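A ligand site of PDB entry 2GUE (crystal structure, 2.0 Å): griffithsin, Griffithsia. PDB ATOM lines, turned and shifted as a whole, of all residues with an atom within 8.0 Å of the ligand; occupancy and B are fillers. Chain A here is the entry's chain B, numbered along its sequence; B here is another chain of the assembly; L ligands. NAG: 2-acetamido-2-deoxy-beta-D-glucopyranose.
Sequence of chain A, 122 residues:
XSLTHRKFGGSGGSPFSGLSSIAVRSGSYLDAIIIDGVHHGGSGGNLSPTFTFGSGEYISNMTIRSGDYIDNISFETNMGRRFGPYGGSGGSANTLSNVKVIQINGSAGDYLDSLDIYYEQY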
ATOM      1  N   SER A  28      17.814 -26.934 -27.032  1.00  0.00           N
ATOM      2  CA  SER A  28      17.571 -25.930 -26.017  1.00  0.00           C
ATOM      3  C   SER A  28      16.309 -25.123 -26.397  1.00  0.00           C
ATOM      4  O   SER A  28      15.768 -24.358 -25.586  1.00  0.00           O
ATOM      5  CB  SER A  28      18.785 -24.995 -25.867  1.00  0.00           C
ATOM      6  OG  SER A  28      18.903 -24.169 -27.006  1.00  0.00           O
ATOM      7  N   TYR A  29      15.856 -25.283 -27.639  1.00  0.00           N
ATOM      8  CA  TYR A  29      14.548 -24.766 -27.997  1.00  0.00           C
ATOM      9  C   TYR A  29      13.664 -25.939 -28.426  1.00  0.00           C
ATOM     10  O   TYR A  29      14.037 -27.104 -28.234  1.00  0.00           O
ATOM     11  CB  TYR A  29      14.634 -23.749 -29.136  1.00  0.00           C
ATOM     12  CG  TYR A  29      15.400 -22.493 -28.792  1.00  0.00           C
ATOM     13  CD1 TYR A  29      14.854 -21.519 -27.928  1.00  0.00           C
ATOM     14  CD2 TYR A  29      16.677 -22.243 -29.368  1.00  0.00           C
ATOM     15  CE1 TYR A  29      15.549 -20.333 -27.612  1.00  0.00           C
ATOM     16  CE2 TYR A  29      17.381 -21.054 -29.055  1.00  0.00           C
ATOM     17  CZ  TYR A  29      16.814 -20.105 -28.174  1.00  0.00           C
ATOM     18  OH  TYR A  29      17.497 -18.924 -27.863  1.00  0.00           O
ATOM     19  N   LEU A  30      12.485 -25.590 -28.948  1.00  0.00           N
ATOM     20  CA  LEU A  30      11.648 -26.484 -29.745  1.00  0.00           C
ATOM     21  C   LEU A  30      11.887 -26.211 -31.209  1.00  0.00           C
ATOM     22  O   LEU A  30      11.610 -25.124 -31.654  1.00  0.00           O
ATOM     23  CB  LEU A  30      10.130 -26.355 -29.401  1.00  0.00           C
ATOM     24  CG  LEU A  30       9.967 -27.491 -28.391  1.00  0.00           C
ATOM     25  CD1 LEU A  30      10.313 -27.066 -26.957  1.00  0.00           C
ATOM     26  CD2 LEU A  30       8.620 -28.144 -28.462  1.00  0.00           C
ATOM     27  N   ARG A  65       7.300 -23.014 -21.545  1.00  0.00           N
ATOM     28  CA  ARG A  65       8.211 -21.835 -21.411  1.00  0.00           C
ATOM     29  C   ARG A  65       8.393 -21.217 -22.791  1.00  0.00           C
ATOM     30  O   ARG A  65       8.652 -21.929 -23.763  1.00  0.00           O
ATOM     31  CB  ARG A  65       9.561 -22.229 -20.814  1.00  0.00           C
ATOM     32  CG  ARG A  65       9.563 -23.138 -19.556  1.00  0.00           C
ATOM     33  CD  ARG A  65      11.011 -23.293 -19.017  1.00  0.00           C
ATOM     34  NE  ARG A  65      11.577 -21.954 -18.803  1.00  0.00           N
ATOM     35  CZ  ARG A  65      11.435 -21.226 -17.689  1.00  0.00           C
ATOM     36  NH1 ARG A  65      10.785 -21.726 -16.629  1.00  0.00           N
ATOM     37  NH2 ARG A  65      11.952 -19.997 -17.638  1.00  0.00           N
ATOM     38  N   SER A  66       8.240 -19.906 -22.895  1.00  0.00           N
ATOM     39  CA  SER A  66       8.255 -19.258 -24.208  1.00  0.00           C
ATOM     40  C   SER A  66       8.641 -17.752 -24.191  1.00  0.00           C
ATOM     41  O   SER A  66       8.529 -17.068 -23.167  1.00  0.00           O
ATOM     42  CB  SER A  66       6.892 -19.428 -24.861  1.00  0.00           C
ATOM     43  OG  SER A  66       5.906 -18.609 -24.233  1.00  0.00           O
ATOM     44  N   GLY A  67       9.093 -17.256 -25.341  1.00  0.00           N
ATOM     45  CA  GLY A  67       9.629 -15.910 -25.485  1.00  0.00           C
ATOM     46  C   GLY A  67       9.242 -15.488 -26.865  1.00  0.00           C
ATOM     47  O   GLY A  67       8.072 -15.326 -27.133  1.00  0.00           O
ATOM     48  N   ASP A  68      10.219 -15.313 -27.753  1.00  0.00           N
ATOM     49  CA  ASP A  68       9.959 -15.185 -29.204  1.00  0.00           C
ATOM     50  C   ASP A  68       9.767 -16.572 -29.841  1.00  0.00           C
ATOM     51  O   ASP A  68       9.173 -16.718 -30.902  1.00  0.00           O
ATOM     52  CB  ASP A  68      11.094 -14.438 -29.911  1.00  0.00           C
ATOM     53  CG  ASP A  68      11.024 -12.933 -29.742  1.00  0.00           C
ATOM     54  OD1 ASP A  68      10.400 -12.443 -28.770  1.00  0.00           O
ATOM     55  OD2 ASP A  68      11.594 -12.223 -30.603  1.00  0.00           O
ATOM     56  N   TYR A  69      10.271 -17.610 -29.176  1.00  0.00           N
ATOM     57  CA  TYR A  69      10.065 -19.002 -29.626  1.00  0.00           C
ATOM     58  C   TYR A  69       9.476 -19.818 -28.507  1.00  0.00           C
ATOM     59  O   TYR A  69       9.319 -19.308 -27.391  1.00  0.00           O
ATOM     60  CB  TYR A  69      11.366 -19.602 -30.215  1.00  0.00           C
ATOM     61  CG  TYR A  69      11.693 -18.885 -31.500  1.00  0.00           C
ATOM     62  CD1 TYR A  69      12.431 -17.708 -31.475  1.00  0.00           C
ATOM     63  CD2 TYR A  69      11.191 -19.326 -32.723  1.00  0.00           C
ATOM     64  CE1 TYR A  69      12.693 -16.984 -32.642  1.00  0.00           C
ATOM     65  CE2 TYR A  69      11.441 -18.608 -33.896  1.00  0.00           C
ATOM     66  CZ  TYR A  69      12.190 -17.428 -33.841  1.00  0.00           C
ATOM     67  OH  TYR A  69      12.465 -16.681 -34.989  1.00  0.00           O
ATOM     68  N   ILE A  70       9.137 -21.079 -28.798  1.00  0.00           N
ATOM     69  CA  ILE A  70       8.826 -22.031 -27.751  1.00  0.00           C
ATOM     70  C   ILE A  70      10.096 -22.699 -27.210  1.00  0.00           C
ATOM     71  O   ILE A  70      10.848 -23.335 -27.969  1.00  0.00           O
ATOM     72  CB  ILE A  70       7.809 -23.136 -28.230  1.00  0.00           C
ATOM     73  CG1 ILE A  70       6.511 -22.506 -28.723  1.00  0.00           C
ATOM     74  CG2 ILE A  70       7.580 -24.162 -27.127  1.00  0.00           C
ATOM     75  CD1 ILE A  70       5.585 -22.025 -27.685  1.00  0.00           C
ATOM     76  N   ASP A  71      10.301 -22.600 -25.882  1.00  0.00           N
ATOM     77  CA  ASP A  71      11.553 -23.009 -25.261  1.00  0.00           C
ATOM     78  C   ASP A  71      11.454 -24.377 -24.651  1.00  0.00           C
ATOM     79  O   ASP A  71      12.447 -25.129 -24.595  1.00  0.00           O
ATOM     80  CB  ASP A  71      11.930 -22.002 -24.115  1.00  0.00           C
ATOM     81  CG  ASP A  71      12.705 -20.790 -24.628  1.00  0.00           C
ATOM     82  OD1 ASP A  71      12.067 -19.801 -25.073  1.00  0.00           O
ATOM     83  OD2 ASP A  71      13.978 -20.828 -24.559  1.00  0.00           O
ATOM     84  N   ASN A  72      10.229 -24.703 -24.214  1.00  0.00           N
ATOM     85  CA  ASN A  72       9.966 -25.905 -23.474  1.00  0.00           C
ATOM     86  C   ASN A  72       8.438 -26.203 -23.465  1.00  0.00           C
ATOM     87  O   ASN A  72       7.626 -25.280 -23.605  1.00  0.00           O
ATOM     88  CB  ASN A  72      10.501 -25.722 -22.062  1.00  0.00           C
ATOM     89  CG  ASN A  72      10.791 -27.003 -21.385  1.00  0.00           C
ATOM     90  OD1 ASN A  72       9.892 -27.825 -21.163  1.00  0.00           O
ATOM     91  ND2 ASN A  72      12.082 -27.212 -21.060  1.00  0.00           N
ATOM     92  N   GLY A  88      14.847 -26.124 -23.675  1.00  0.00           N
ATOM     93  CA  GLY A  88      15.694 -25.397 -22.725  1.00  0.00           C
ATOM     94  C   GLY A  88      15.018 -24.839 -21.475  1.00  0.00           C
ATOM     95  O   GLY A  88      13.795 -24.987 -21.268  1.00  0.00           O
ATOM     96  N   SER A  89      15.833 -24.209 -20.608  1.00  0.00           N
ATOM     97  CA  SER A  89      15.349 -23.460 -19.430  1.00  0.00           C
ATOM     98  C   SER A  89      15.026 -21.993 -19.741  1.00  0.00           C
ATOM     99  O   SER A  89      14.628 -21.224 -18.813  1.00  0.00           O
ATOM    100  CB  SER A  89      16.309 -23.594 -18.241  1.00  0.00           C
ATOM    101  OG  SER A  89      17.644 -23.967 -18.637  1.00  0.00           O
ATOM    102  N   GLY A  90      15.190 -21.562 -20.996  1.00  0.00           N
ATOM    103  CA  GLY A  90      14.854 -20.190 -21.339  1.00  0.00           C
ATOM    104  C   GLY A  90      13.371 -19.833 -21.337  1.00  0.00           C
ATOM    105  O   GLY A  90      12.518 -20.678 -21.038  1.00  0.00           O
ATOM    106  N   GLY A  91      13.062 -18.575 -21.680  1.00  0.00           N
ATOM    107  CA  GLY A  91      11.686 -18.091 -21.778  1.00  0.00           C
ATOM    108  C   GLY A  91      10.960 -17.935 -20.442  1.00  0.00           C
ATOM    109  O   GLY A  91      11.513 -18.247 -19.363  1.00  0.00           O
ATOM    110  N   SER A  92       9.735 -17.386 -20.509  1.00  0.00           N
ATOM    111  CA  SER A  92       8.789 -17.255 -19.362  1.00  0.00           C
ATOM    112  C   SER A  92       7.948 -18.571 -19.168  1.00  0.00           C
ATOM    113  O   SER A  92       7.565 -19.173 -20.147  1.00  0.00           O
ATOM    114  CB  SER A  92       7.866 -16.043 -19.648  1.00  0.00           C
ATOM    115  OG  SER A  92       6.659 -16.044 -18.855  1.00  0.00           O
ATOM    116  N   TYR A 111      12.203 -23.335 -36.594  1.00  0.00           N
ATOM    117  CA  TYR A 111      11.985 -23.522 -35.164  1.00  0.00           C
ATOM    118  C   TYR A 111      10.487 -23.398 -34.857  1.00  0.00           C
ATOM    119  O   TYR A 111       9.717 -22.822 -35.632  1.00  0.00           O
ATOM    120  CB  TYR A 111      12.823 -22.466 -34.385  1.00  0.00           C
ATOM    121  CG  TYR A 111      14.328 -22.591 -34.704  1.00  0.00           C
ATOM    122  CD1 TYR A 111      15.121 -23.502 -34.009  1.00  0.00           C
ATOM    123  CD2 TYR A 111      14.917 -21.822 -35.734  1.00  0.00           C
ATOM    124  CE1 TYR A 111      16.471 -23.676 -34.307  1.00  0.00           C
ATOM    125  CE2 TYR A 111      16.299 -21.967 -36.043  1.00  0.00           C
ATOM    126  CZ  TYR A 111      17.061 -22.906 -35.303  1.00  0.00           C
ATOM    127  OH  TYR A 111      18.413 -23.093 -35.574  1.00  0.00           O
ATOM    128  N   LEU A 112      10.057 -23.912 -33.717  1.00  0.00           N
ATOM    129  CA  LEU A 112       8.662 -23.678 -33.331  1.00  0.00           C
ATOM    130  C   LEU A 112       8.512 -22.250 -32.763  1.00  0.00           C
ATOM    131  O   LEU A 112       8.982 -21.980 -31.668  1.00  0.00           O
ATOM    132  CB  LEU A 112       8.176 -24.755 -32.359  1.00  0.00           C
ATOM    133  CG  LEU A 112       6.722 -24.607 -31.837  1.00  0.00           C
ATOM    134  CD1 LEU A 112       5.715 -24.794 -32.968  1.00  0.00           C
ATOM    135  CD2 LEU A 112       6.444 -25.590 -30.751  1.00  0.00           C
ATOM    136  N   ASP A 113       7.868 -21.344 -33.499  1.00  0.00           N
ATOM    137  CA  ASP A 113       7.792 -19.951 -33.072  1.00  0.00           C
ATOM    138  C   ASP A 113       6.707 -19.760 -31.993  1.00  0.00           C
ATOM    139  O   ASP A 113       6.964 -19.141 -30.930  1.00  0.00           O
ATOM    140  CB  ASP A 113       7.439 -19.023 -34.263  1.00  0.00           C
ATOM    141  CG  ASP A 113       8.545 -18.926 -35.345  1.00  0.00           C
ATOM    142  OD1 ASP A 113       8.796 -19.914 -36.074  1.00  0.00           O
ATOM    143  OD2 ASP A 113       9.130 -17.828 -35.479  1.00  0.00           O
ATOM    144  N   GLY B   9       4.563 -17.934 -27.290  1.00  0.00           N
ATOM    145  CA  GLY B   9       5.675 -17.673 -28.233  1.00  0.00           C
ATOM    146  C   GLY B   9       5.517 -16.340 -28.960  1.00  0.00           C
ATOM    147  O   GLY B   9       4.750 -15.454 -28.493  1.00  0.00           O
ATOM    148  N   GLY B  10       6.217 -16.201 -30.106  1.00  0.00           N
ATOM    149  CA  GLY B  10       6.240 -14.960 -30.932  1.00  0.00           C
ATOM    150  C   GLY B  10       5.481 -14.879 -32.256  1.00  0.00           C
ATOM    151  O   GLY B  10       4.532 -15.666 -32.514  1.00  0.00           O
HETATM  152  C1  NAG L   1      14.600 -17.620 -24.231  1.00  0.00           C
HETATM  153  C2  NAG L   1      14.810 -16.106 -24.042  1.00  0.00           C
HETATM  154  C3  NAG L   1      13.571 -15.310 -24.538  1.00  0.00           C
HETATM  155  C4  NAG L   1      13.443 -15.688 -26.032  1.00  0.00           C
HETATM  156  C5  NAG L   1      13.036 -17.148 -25.962  1.00  0.00           C
HETATM  157  C6  NAG L   1      12.364 -17.704 -27.211  1.00  0.00           C
HETATM  158  C7  NAG L   1      16.283 -15.234 -22.290  1.00  0.00           C
HETATM  159  C8  NAG L   1      17.156 -14.637 -23.366  1.00  0.00           C
HETATM  160  N2  NAG L   1      15.157 -15.913 -22.628  1.00  0.00           N
HETATM  161  O1  NAG L   1      15.776 -18.376 -23.873  1.00  0.00           O
HETATM  162  O3  NAG L   1      13.649 -13.905 -24.331  1.00  0.00           O
HETATM  163  O4  NAG L   1      12.582 -14.894 -26.859  1.00  0.00           O
HETATM  164  O5  NAG L   1      14.205 -17.889 -25.586  1.00  0.00           O
HETATM  165  O6  NAG L   1      13.249 -17.671 -28.337  1.00  0.00           O
HETATM  166  O7  NAG L   1      16.588 -15.076 -21.120  1.00  0.00           O
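The guanidinium group (NE) of Arg 65 sits at hydrogen-bond distance from the backbone carbonyl oxygen (O) of Gly 90 (2.7 Å). O of Asp 71 is in hydrogen-bond range of N of Gly 88 (2.8 Å). The backbone carbonyl oxygen of Asp 68 sits at hydrogen-bond distance from the backbone NH of Gly 10 of chain B (3.1 Å). The backbone NH of Asp 71 lies within hydrogen-bond range of the backbone carbonyl oxygen of Arg 65. NH2 of Arg 65 is in hydrogen-bond range of O of Gly 91, 2.5 Å away.
Tyr 29 touches the ligand. Gly 67 touches the ligand. Gly 90 touches the ligand. Hydrophobic or aromatic side chains that line the ligand: Tyr 29 and Tyr 69. The nearest printed residue that does not touch the ligand is Ser 66 (4.8 Å).
N of Gly 91 lies close to O1 of the ligand. N of Asp 68 lies within hydrogen-bond range of O4 of the ligand (2.6 Å). OD2 of Asp 71 lies within hydrogen-bond range of O1 of the ligand, 3.1 Å away. The backbone NH (N) of Tyr 69 sits close to an oxygen (O6) of the ligand, 3.1 Å away.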
